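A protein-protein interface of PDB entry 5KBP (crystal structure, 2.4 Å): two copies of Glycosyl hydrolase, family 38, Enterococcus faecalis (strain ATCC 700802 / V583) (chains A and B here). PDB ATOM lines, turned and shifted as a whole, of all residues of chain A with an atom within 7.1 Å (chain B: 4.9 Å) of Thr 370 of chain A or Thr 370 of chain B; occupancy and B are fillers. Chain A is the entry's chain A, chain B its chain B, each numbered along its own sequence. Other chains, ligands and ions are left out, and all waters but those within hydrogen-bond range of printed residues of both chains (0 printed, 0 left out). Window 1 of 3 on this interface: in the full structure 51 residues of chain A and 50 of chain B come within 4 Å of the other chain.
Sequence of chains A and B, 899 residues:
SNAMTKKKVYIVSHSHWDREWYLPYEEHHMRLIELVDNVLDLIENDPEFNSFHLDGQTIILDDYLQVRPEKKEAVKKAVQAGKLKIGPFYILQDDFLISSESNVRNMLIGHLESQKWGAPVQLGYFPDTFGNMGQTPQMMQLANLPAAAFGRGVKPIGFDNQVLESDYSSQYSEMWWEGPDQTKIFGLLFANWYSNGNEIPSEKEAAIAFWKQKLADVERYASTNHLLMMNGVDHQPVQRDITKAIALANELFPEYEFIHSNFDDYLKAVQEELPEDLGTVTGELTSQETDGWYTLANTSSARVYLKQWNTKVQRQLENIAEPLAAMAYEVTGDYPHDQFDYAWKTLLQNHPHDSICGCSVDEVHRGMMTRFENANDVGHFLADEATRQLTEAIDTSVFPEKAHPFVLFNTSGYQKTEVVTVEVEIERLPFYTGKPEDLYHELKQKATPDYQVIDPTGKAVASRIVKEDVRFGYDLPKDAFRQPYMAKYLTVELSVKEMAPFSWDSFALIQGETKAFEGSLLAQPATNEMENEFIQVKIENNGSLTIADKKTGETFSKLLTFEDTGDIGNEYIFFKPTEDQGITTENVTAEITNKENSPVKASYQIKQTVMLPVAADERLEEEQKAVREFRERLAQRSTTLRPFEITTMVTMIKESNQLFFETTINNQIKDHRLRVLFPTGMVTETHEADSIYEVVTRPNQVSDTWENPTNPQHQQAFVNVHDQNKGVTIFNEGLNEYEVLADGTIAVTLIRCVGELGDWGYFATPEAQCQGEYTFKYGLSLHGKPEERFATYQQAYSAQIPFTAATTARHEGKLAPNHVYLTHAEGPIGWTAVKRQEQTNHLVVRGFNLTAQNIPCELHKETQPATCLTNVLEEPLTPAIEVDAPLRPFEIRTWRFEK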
ATOM      1  N   GLU A  26      16.917 -40.301  10.873  1.00  0.00           N
ATOM      2  CA  GLU A  26      17.971 -41.309  10.854  1.00  0.00           C
ATOM      3  C   GLU A  26      17.408 -42.723  10.769  1.00  0.00           C
ATOM      4  O   GLU A  26      18.096 -43.628  10.286  1.00  0.00           O
ATOM      5  CB  GLU A  26      18.864 -41.161  12.084  1.00  0.00           C
ATOM      6  CG  GLU A  26      19.724 -39.904  12.082  1.00  0.00           C
ATOM      7  CD  GLU A  26      20.782 -39.897  10.986  1.00  0.00           C
ATOM      8  OE1 GLU A  26      21.366 -38.821  10.737  1.00  0.00           O
ATOM      9  OE2 GLU A  26      21.038 -40.959  10.378  1.00  0.00           O
ATOM     10  N   THR A 346      21.584 -27.140   2.070  1.00  0.00           N
ATOM     11  CA  THR A 346      20.998 -27.182   3.405  1.00  0.00           C
ATOM     12  C   THR A 346      19.530 -26.774   3.371  1.00  0.00           C
ATOM     13  O   THR A 346      18.693 -27.380   4.050  1.00  0.00           O
ATOM     14  CB  THR A 346      21.786 -26.276   4.352  1.00  0.00           C
ATOM     15  OG1 THR A 346      23.147 -26.719   4.421  1.00  0.00           O
ATOM     16  CG2 THR A 346      21.177 -26.296   5.748  1.00  0.00           C
ATOM     17  N   ASN A 350      15.219 -29.216   3.403  1.00  0.00           N
ATOM     18  CA  ASN A 350      13.903 -28.977   3.980  1.00  0.00           C
ATOM     19  C   ASN A 350      12.802 -28.951   2.929  1.00  0.00           C
ATOM     20  O   ASN A 350      11.635 -28.749   3.278  1.00  0.00           O
ATOM     21  CB  ASN A 350      13.889 -27.657   4.759  1.00  0.00           C
ATOM     22  CG  ASN A 350      14.530 -27.779   6.123  1.00  0.00           C
ATOM     23  OD1 ASN A 350      14.752 -28.882   6.618  1.00  0.00           O
ATOM     24  ND2 ASN A 350      14.822 -26.643   6.745  1.00  0.00           N
ATOM     25  N   GLU A 363       9.658 -35.242  15.357  1.00  0.00           N
ATOM     26  CA  GLU A 363      11.117 -35.272  15.327  1.00  0.00           C
ATOM     27  C   GLU A 363      11.660 -34.771  13.997  1.00  0.00           C
ATOM     28  O   GLU A 363      12.722 -34.138  13.959  1.00  0.00           O
ATOM     29  CB  GLU A 363      11.626 -36.688  15.602  1.00  0.00           C
ATOM     30  CG  GLU A 363      11.269 -37.238  16.975  1.00  0.00           C
ATOM     31  CD  GLU A 363       9.851 -37.772  17.044  1.00  0.00           C
ATOM     32  OE1 GLU A 363       9.181 -37.554  18.075  1.00  0.00           O
ATOM     33  OE2 GLU A 363       9.406 -38.405  16.064  1.00  0.00           O
ATOM     34  N   HIS A 365      10.339 -32.442  11.978  1.00  0.00           N
ATOM     35  CA  HIS A 365      10.187 -31.006  11.778  1.00  0.00           C
ATOM     36  C   HIS A 365      11.030 -30.188  12.747  1.00  0.00           C
ATOM     37  O   HIS A 365      11.419 -29.062  12.418  1.00  0.00           O
ATOM     38  CB  HIS A 365       8.711 -30.623  11.882  1.00  0.00           C
ATOM     39  CG  HIS A 365       7.867 -31.210  10.795  1.00  0.00           C
ATOM     40  ND1 HIS A 365       6.747 -31.971  11.049  1.00  0.00           N
ATOM     41  CD2 HIS A 365       7.989 -31.160   9.447  1.00  0.00           C
ATOM     42  CE1 HIS A 365       6.208 -32.354   9.906  1.00  0.00           C
ATOM     43  NE2 HIS A 365       6.945 -31.880   8.918  1.00  0.00           N
ATOM     44  N   ARG A 366      11.323 -30.721  13.935  1.00  0.00           N
ATOM     45  CA  ARG A 366      12.320 -30.076  14.783  1.00  0.00           C
ATOM     46  C   ARG A 366      13.694 -30.118  14.132  1.00  0.00           C
ATOM     47  O   ARG A 366      14.494 -29.193  14.308  1.00  0.00           O
ATOM     48  CB  ARG A 366      12.364 -30.735  16.163  1.00  0.00           C
ATOM     49  CG  ARG A 366      11.095 -30.555  16.978  1.00  0.00           C
ATOM     50  CD  ARG A 366      11.352 -30.768  18.460  1.00  0.00           C
ATOM     51  NE  ARG A 366      11.920 -32.084  18.732  1.00  0.00           N
ATOM     52  CZ  ARG A 366      11.197 -33.177  18.953  1.00  0.00           C
ATOM     53  NH1 ARG A 366       9.873 -33.111  18.934  1.00  0.00           N
ATOM     54  NH2 ARG A 366      11.797 -34.335  19.193  1.00  0.00           N
ATOM     55  N   GLY A 367      13.979 -31.174  13.368  1.00  0.00           N
ATOM     56  CA  GLY A 367      15.224 -31.228  12.623  1.00  0.00           C
ATOM     57  C   GLY A 367      15.249 -30.280  11.443  1.00  0.00           C
ATOM     58  O   GLY A 367      16.320 -29.820  11.036  1.00  0.00           O
ATOM     59  N   MET A 368      14.079 -29.978  10.872  1.00  0.00           N
ATOM     60  CA  MET A 368      14.008 -28.986   9.804  1.00  0.00           C
ATOM     61  C   MET A 368      14.334 -27.593  10.322  1.00  0.00           C
ATOM     62  O   MET A 368      14.935 -26.789   9.600  1.00  0.00           O
ATOM     63  CB  MET A 368      12.620 -28.991   9.161  1.00  0.00           C
ATOM     64  CG  MET A 368      12.271 -30.262   8.413  1.00  0.00           C
ATOM     65  SD  MET A 368      10.630 -30.160   7.673  1.00  0.00           S
ATOM     66  CE  MET A 368      10.818 -28.702   6.647  1.00  0.00           C
ATOM     67  N   MET A 369      13.933 -27.285  11.558  1.00  0.00           N
ATOM     68  CA  MET A 369      14.250 -25.984  12.137  1.00  0.00           C
ATOM     69  C   MET A 369      15.755 -25.785  12.254  1.00  0.00           C
ATOM     70  O   MET A 369      16.260 -24.676  12.040  1.00  0.00           O
ATOM     71  CB  MET A 369      13.584 -25.841  13.505  1.00  0.00           C
ATOM     72  CG  MET A 369      12.079 -25.610  13.463  1.00  0.00           C
ATOM     73  SD  MET A 369      11.622 -23.928  12.995  1.00  0.00           S
ATOM     74  CE  MET A 369      11.249 -24.138  11.265  1.00  0.00           C
ATOM     75  N   THR A 370      16.490 -26.849  12.589  1.00  0.00           N
ATOM     76  CA  THR A 370      17.945 -26.753  12.644  1.00  0.00           C
ATOM     77  C   THR A 370      18.523 -26.447  11.268  1.00  0.00           C
ATOM     78  O   THR A 370      19.426 -25.611  11.137  1.00  0.00           O
ATOM     79  CB  THR A 370      18.539 -28.048  13.201  1.00  0.00           C
ATOM     80  OG1 THR A 370      18.144 -28.211  14.569  1.00  0.00           O
ATOM     81  CG2 THR A 370      20.061 -28.023  13.119  1.00  0.00           C
ATOM     82  N   ARG A 371      18.006 -27.106  10.228  1.00  0.00           N
ATOM     83  CA  ARG A 371      18.451 -26.813   8.870  1.00  0.00           C
ATOM     84  C   ARG A 371      18.121 -25.377   8.482  1.00  0.00           C
ATOM     85  O   ARG A 371      18.933 -24.696   7.845  1.00  0.00           O
ATOM     86  CB  ARG A 371      17.813 -27.788   7.882  1.00  0.00           C
ATOM     87  CG  ARG A 371      18.072 -29.258   8.175  1.00  0.00           C
ATOM     88  CD  ARG A 371      17.739 -30.105   6.957  1.00  0.00           C
ATOM     89  NE  ARG A 371      17.814 -31.537   7.227  1.00  0.00           N
ATOM     90  CZ  ARG A 371      16.757 -32.312   7.446  1.00  0.00           C
ATOM     91  NH1 ARG A 371      16.917 -33.608   7.679  1.00  0.00           N
ATOM     92  NH2 ARG A 371      15.537 -31.792   7.429  1.00  0.00           N
ATOM     93  N   PHE A 372      16.929 -24.905   8.854  1.00  0.00           N
ATOM     94  CA  PHE A 372      16.551 -23.524   8.568  1.00  0.00           C
ATOM     95  C   PHE A 372      17.487 -22.543   9.263  1.00  0.00           C
ATOM     96  O   PHE A 372      17.946 -21.570   8.655  1.00  0.00           O
ATOM     97  CB  PHE A 372      15.102 -23.281   8.993  1.00  0.00           C
ATOM     98  CG  PHE A 372      14.090 -23.664   7.950  1.00  0.00           C
ATOM     99  CD1 PHE A 372      14.252 -23.271   6.633  1.00  0.00           C
ATOM    100  CD2 PHE A 372      12.977 -24.418   8.286  1.00  0.00           C
ATOM    101  CE1 PHE A 372      13.323 -23.621   5.673  1.00  0.00           C
ATOM    102  CE2 PHE A 372      12.045 -24.769   7.331  1.00  0.00           C
ATOM    103  CZ  PHE A 372      12.219 -24.371   6.023  1.00  0.00           C
ATOM    104  N   GLU A 373      17.779 -22.785  10.543  1.00  0.00           N
ATOM    105  CA  GLU A 373      18.690 -21.912  11.277  1.00  0.00           C
ATOM    106  C   GLU A 373      20.068 -21.883  10.628  1.00  0.00           C
ATOM    107  O   GLU A 373      20.667 -20.812  10.472  1.00  0.00           O
ATOM    108  CB  GLU A 373      18.801 -22.370  12.732  1.00  0.00           C
ATOM    109  CG  GLU A 373      17.517 -22.251  13.540  1.00  0.00           C
ATOM    110  CD  GLU A 373      17.389 -20.915  14.241  1.00  0.00           C
ATOM    111  OE1 GLU A 373      16.346 -20.680  14.887  1.00  0.00           O
ATOM    112  OE2 GLU A 373      18.334 -20.105  14.152  1.00  0.00           O
ATOM    113  N   ASN A 374      20.581 -23.050  10.232  1.00  0.00           N
ATOM    114  CA  ASN A 374      21.926 -23.123   9.671  1.00  0.00           C
ATOM    115  C   ASN A 374      21.995 -22.451   8.305  1.00  0.00           C
ATOM    116  O   ASN A 374      22.919 -21.677   8.029  1.00  0.00           O
ATOM    117  CB  ASN A 374      22.376 -24.582   9.584  1.00  0.00           C
ATOM    118  CG  ASN A 374      22.664 -25.183  10.946  1.00  0.00           C
ATOM    119  OD1 ASN A 374      22.974 -24.468  11.899  1.00  0.00           O
ATOM    120  ND2 ASN A 374      22.567 -26.504  11.043  1.00  0.00           N
ATOM    121  N   ALA A 375      21.029 -22.741   7.432  1.00  0.00           N
ATOM    122  CA  ALA A 375      21.000 -22.093   6.125  1.00  0.00           C
ATOM    123  C   ALA A 375      20.828 -20.587   6.264  1.00  0.00           C
ATOM    124  O   ALA A 375      21.466 -19.812   5.540  1.00  0.00           O
ATOM    125  CB  ALA A 375      19.880 -22.684   5.269  1.00  0.00           C
ATOM    126  N   ASN A 376      19.981 -20.153   7.200  1.00  0.00           N
ATOM    127  CA  ASN A 376      19.743 -18.724   7.384  1.00  0.00           C
ATOM    128  C   ASN A 376      20.997 -18.012   7.878  1.00  0.00           C
ATOM    129  O   ASN A 376      21.292 -16.891   7.450  1.00  0.00           O
ATOM    130  CB  ASN A 376      18.579 -18.508   8.353  1.00  0.00           C
ATOM    131  CG  ASN A 376      18.178 -17.050   8.470  1.00  0.00           C
ATOM    132  OD1 ASN A 376      17.806 -16.417   7.482  1.00  0.00           O
ATOM    133  ND2 ASN A 376      18.232 -16.516   9.684  1.00  0.00           N
ATOM    134  N   ASP A 377      21.753 -18.652   8.773  1.00  0.00           N
ATOM    135  CA  ASP A 377      22.960 -18.024   9.300  1.00  0.00           C
ATOM    136  C   ASP A 377      24.056 -17.931   8.246  1.00  0.00           C
ATOM    137  O   ASP A 377      24.863 -16.994   8.278  1.00  0.00           O
ATOM    138  CB  ASP A 377      23.461 -18.788  10.523  1.00  0.00           C
ATOM    139  CG  ASP A 377      22.504 -18.701  11.695  1.00  0.00           C
ATOM    140  OD1 ASP A 377      21.726 -17.726  11.756  1.00  0.00           O
ATOM    141  OD2 ASP A 377      22.530 -19.605  12.555  1.00  0.00           O
ATOM    142  N   ARG B 366      20.386 -25.573  20.841  1.00  0.00           N
ATOM    143  CA  ARG B 366      19.278 -26.137  20.078  1.00  0.00           C
ATOM    144  C   ARG B 366      19.794 -27.077  18.997  1.00  0.00           C
ATOM    145  O   ARG B 366      19.215 -28.142  18.758  1.00  0.00           O
ATOM    146  CB  ARG B 366      18.431 -25.024  19.458  1.00  0.00           C
ATOM    147  CG  ARG B 366      17.584 -24.250  20.453  1.00  0.00           C
ATOM    148  CD  ARG B 366      16.417 -23.556  19.764  1.00  0.00           C
ATOM    149  NE  ARG B 366      16.857 -22.559  18.793  1.00  0.00           N
ATOM    150  CZ  ARG B 366      17.091 -21.285  19.090  1.00  0.00           C
ATOM    151  NH1 ARG B 366      16.928 -20.856  20.335  1.00  0.00           N
ATOM    152  NH2 ARG B 366      17.488 -20.441  18.148  1.00  0.00           N
ATOM    153  N   GLY B 367      20.895 -26.701  18.341  1.00  0.00           N
ATOM    154  CA  GLY B 367      21.497 -27.582  17.357  1.00  0.00           C
ATOM    155  C   GLY B 367      22.059 -28.851  17.964  1.00  0.00           C
ATOM    156  O   GLY B 367      22.053 -29.904  17.321  1.00  0.00           O
ATOM    157  N   MET B 368      22.553 -28.776  19.203  1.00  0.00           N
ATOM    158  CA  MET B 368      23.043 -29.975  19.875  1.00  0.00           C
ATOM    159  C   MET B 368      21.927 -30.979  20.116  1.00  0.00           C
ATOM    160  O   MET B 368      22.168 -32.191  20.085  1.00  0.00           O
ATOM    161  CB  MET B 368      23.703 -29.609  21.204  1.00  0.00           C
ATOM    162  CG  MET B 368      24.977 -28.805  21.083  1.00  0.00           C
ATOM    163  SD  MET B 368      25.661 -28.450  22.711  1.00  0.00           S
ATOM    164  CE  MET B 368      25.847 -30.107  23.366  1.00  0.00           C
ATOM    165  N   MET B 369      20.707 -30.495  20.368  1.00  0.00           N
ATOM    166  CA  MET B 369      19.577 -31.397  20.563  1.00  0.00           C
ATOM    167  C   MET B 369      19.301 -32.216  19.308  1.00  0.00           C
ATOM    168  O   MET B 369      18.960 -33.401  19.397  1.00  0.00           O
ATOM    169  CB  MET B 369      18.335 -30.602  20.974  1.00  0.00           C
ATOM    170  CG  MET B 369      18.407 -29.965  22.360  1.00  0.00           C
ATOM    171  SD  MET B 369      18.020 -31.092  23.719  1.00  0.00           S
ATOM    172  CE  MET B 369      19.612 -31.830  24.054  1.00  0.00           C
ATOM    173  N   THR B 370      19.446 -31.605  18.129  1.00  0.00           N
ATOM    174  CA  THR B 370      19.249 -32.341  16.884  1.00  0.00           C
ATOM    175  C   THR B 370      20.287 -33.446  16.733  1.00  0.00           C
ATOM    176  O   THR B 370      19.957 -34.578  16.362  1.00  0.00           O
ATOM    177  CB  THR B 370      19.306 -31.386  15.692  1.00  0.00           C
ATOM    178  OG1 THR B 370      18.226 -30.449  15.780  1.00  0.00           O
ATOM    179  CG2 THR B 370      19.204 -32.160  14.379  1.00  0.00           C
ATOM    180  N   ARG B 371      21.553 -33.131  17.016  1.00  0.00           N
ATOM    181  CA  ARG B 371      22.600 -34.148  16.970  1.00  0.00           C
ATOM    182  C   ARG B 371      22.347 -35.246  17.994  1.00  0.00           C
ATOM    183  O   ARG B 371      22.565 -36.430  17.713  1.00  0.00           O
ATOM    184  CB  ARG B 371      23.970 -33.512  17.205  1.00  0.00           C
ATOM    185  CG  ARG B 371      24.367 -32.449  16.191  1.00  0.00           C
ATOM    186  CD  ARG B 371      25.860 -32.163  16.269  1.00  0.00           C
ATOM    187  NE  ARG B 371      26.213 -30.886  15.658  1.00  0.00           N
ATOM    188  CZ  ARG B 371      26.435 -29.768  16.342  1.00  0.00           C
ATOM    189  NH1 ARG B 371      26.752 -28.649  15.706  1.00  0.00           N
ATOM    190  NH2 ARG B 371      26.342 -29.771  17.664  1.00  0.00           N
ATOM    191  N   PHE B 372      21.898 -34.869  19.195  1.00  0.00           N
ATOM    192  CA  PHE B 372      21.561 -35.864  20.209  1.00  0.00           C
ATOM    193  C   PHE B 372      20.454 -36.791  19.727  1.00  0.00           C
ATOM    194  O   PHE B 372      20.530 -38.010  19.911  1.00  0.00           O
ATOM    195  CB  PHE B 372      21.148 -35.171  21.508  1.00  0.00           C
ATOM    196  CG  PHE B 372      22.293 -34.876  22.432  1.00  0.00           C
ATOM    197  CD1 PHE B 372      23.276 -35.823  22.663  1.00  0.00           C
ATOM    198  CD2 PHE B 372      22.386 -33.653  23.073  1.00  0.00           C
ATOM    199  CE1 PHE B 372      24.329 -35.554  23.513  1.00  0.00           C
ATOM    200  CE2 PHE B 372      23.438 -33.376  23.926  1.00  0.00           C
ATOM    201  CZ  PHE B 372      24.411 -34.329  24.147  1.00  0.00           C
ATOM    202  N   GLU B 373      19.416 -36.228  19.105  1.00  0.00           N
ATOM    203  CA  GLU B 373      18.316 -37.042  18.598  1.00  0.00           C
ATOM    204  C   GLU B 373      18.788 -37.985  17.499  1.00  0.00           C
ATOM    205  O   GLU B 373      18.431 -39.169  17.487  1.00  0.00           O
ATOM    206  CB  GLU B 373      17.194 -36.142  18.083  1.00  0.00           C
ATOM    207  CG  GLU B 373      16.476 -35.340  19.157  1.00  0.00           C
ATOM    208  CD  GLU B 373      15.254 -36.051  19.700  1.00  0.00           C
ATOM    209  OE1 GLU B 373      14.352 -35.361  20.217  1.00  0.00           O
ATOM    210  OE2 GLU B 373      15.194 -37.296  19.607  1.00  0.00           O
ATOM    211  N   ASN B 374      19.596 -37.476  16.565  1.00  0.00           N
ATOM    212  CA  ASN B 374      20.043 -38.290  15.437  1.00  0.00           C
ATOM    213  C   ASN B 374      20.932 -39.436  15.900  1.00  0.00           C
ATOM    214  O   ASN B 374      20.764 -40.582  15.466  1.00  0.00           O
ATOM    215  CB  ASN B 374      20.776 -37.419  14.417  1.00  0.00           C
ATOM    216  CG  ASN B 374      19.859 -36.426  13.733  1.00  0.00           C
ATOM    217  OD1 ASN B 374      18.637 -36.522  13.838  1.00  0.00           O
ATOM    218  ND2 ASN B 374      20.444 -35.472  13.017  1.00  0.00           N
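The guanidinium group of Arg 366 of chain A lies within salt-bridge range of the side-chain carboxylate of Glu 373 of chain B, at 2.9 Å.
OG1 of Thr 370 of chain B sits at hydrogen-bond distance from OG1 of Thr 370 of chain A, at 2.5 Å.
The guanidinium group (NH2) of Arg 366 of chain B is in salt-bridge range of the side-chain carboxylate (OE1) of Glu 373 of chain A (3.5 Å).
O of Thr 370 of chain A is in hydrogen-bond range of ND2 of Asn 374 of chain A, at 3.3 Å.
OD1 of Asn 374 of chain B sits close to O of Thr 370 of chain B (3.4 Å).
Among the printed residues, merely in contact across the chains: Glu 26 of chain A with Asn 374 of chain B (3.6 Å).
Thr 370 of chain B touches one residue of chain A.
Of the printed residues of chain B, Glu 373 of chain A touches Arg 366.
Printed residues of chain A within 4 Å of Arg 366 of chain B: Glu 373 (3.5 Å).
Printed residues of chain A within 4 Å of Asn 374 of chain B: Glu 26.
Printed residues of chain B within 4 Å of Glu 26 of chain A: Asn 374.
Of the printed residues of chain B, Arg 366 of chain A touches Glu 373 (2.9 Å).
The nearest residue of chain B that does not touch Thr 370 of chain A is Arg 366 of chain B (4.3 Å).
The nearest printed residue of chain B that does not touch Arg 366 of chain A is Thr 370 of chain B (4.2 Å).
Of the 9 printed residues of chain B, 4 touch a printed residue of chain A.
Along chain B the printed residues that touch a printed residue of chain A span positions 366 to 374.
Of the 17 printed residues of chain A, 4 touch a printed residue of chain B.
Among the printed residues, 4 pairs touch across the chains.
Among the printed residues, Asp or Glu carboxylates within 4 Å of a Lys or Arg side-chain nitrogen of the other chain: Arg 366 of chain A with Glu 373 of chain B and Glu 373 of chain A with Arg 366 of chain B.
Arg 366 of chain A touches Glu 373 of chain B, and with the chains exchanged Glu 373 of chain A touches Arg 366 of chain B.
Thr 370 of chain A touches its own counterpart, Thr 370 of chain B.
Positions printed for both chains: 366, 367, 368, 369, 370, 371, 372, 373 and 374.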
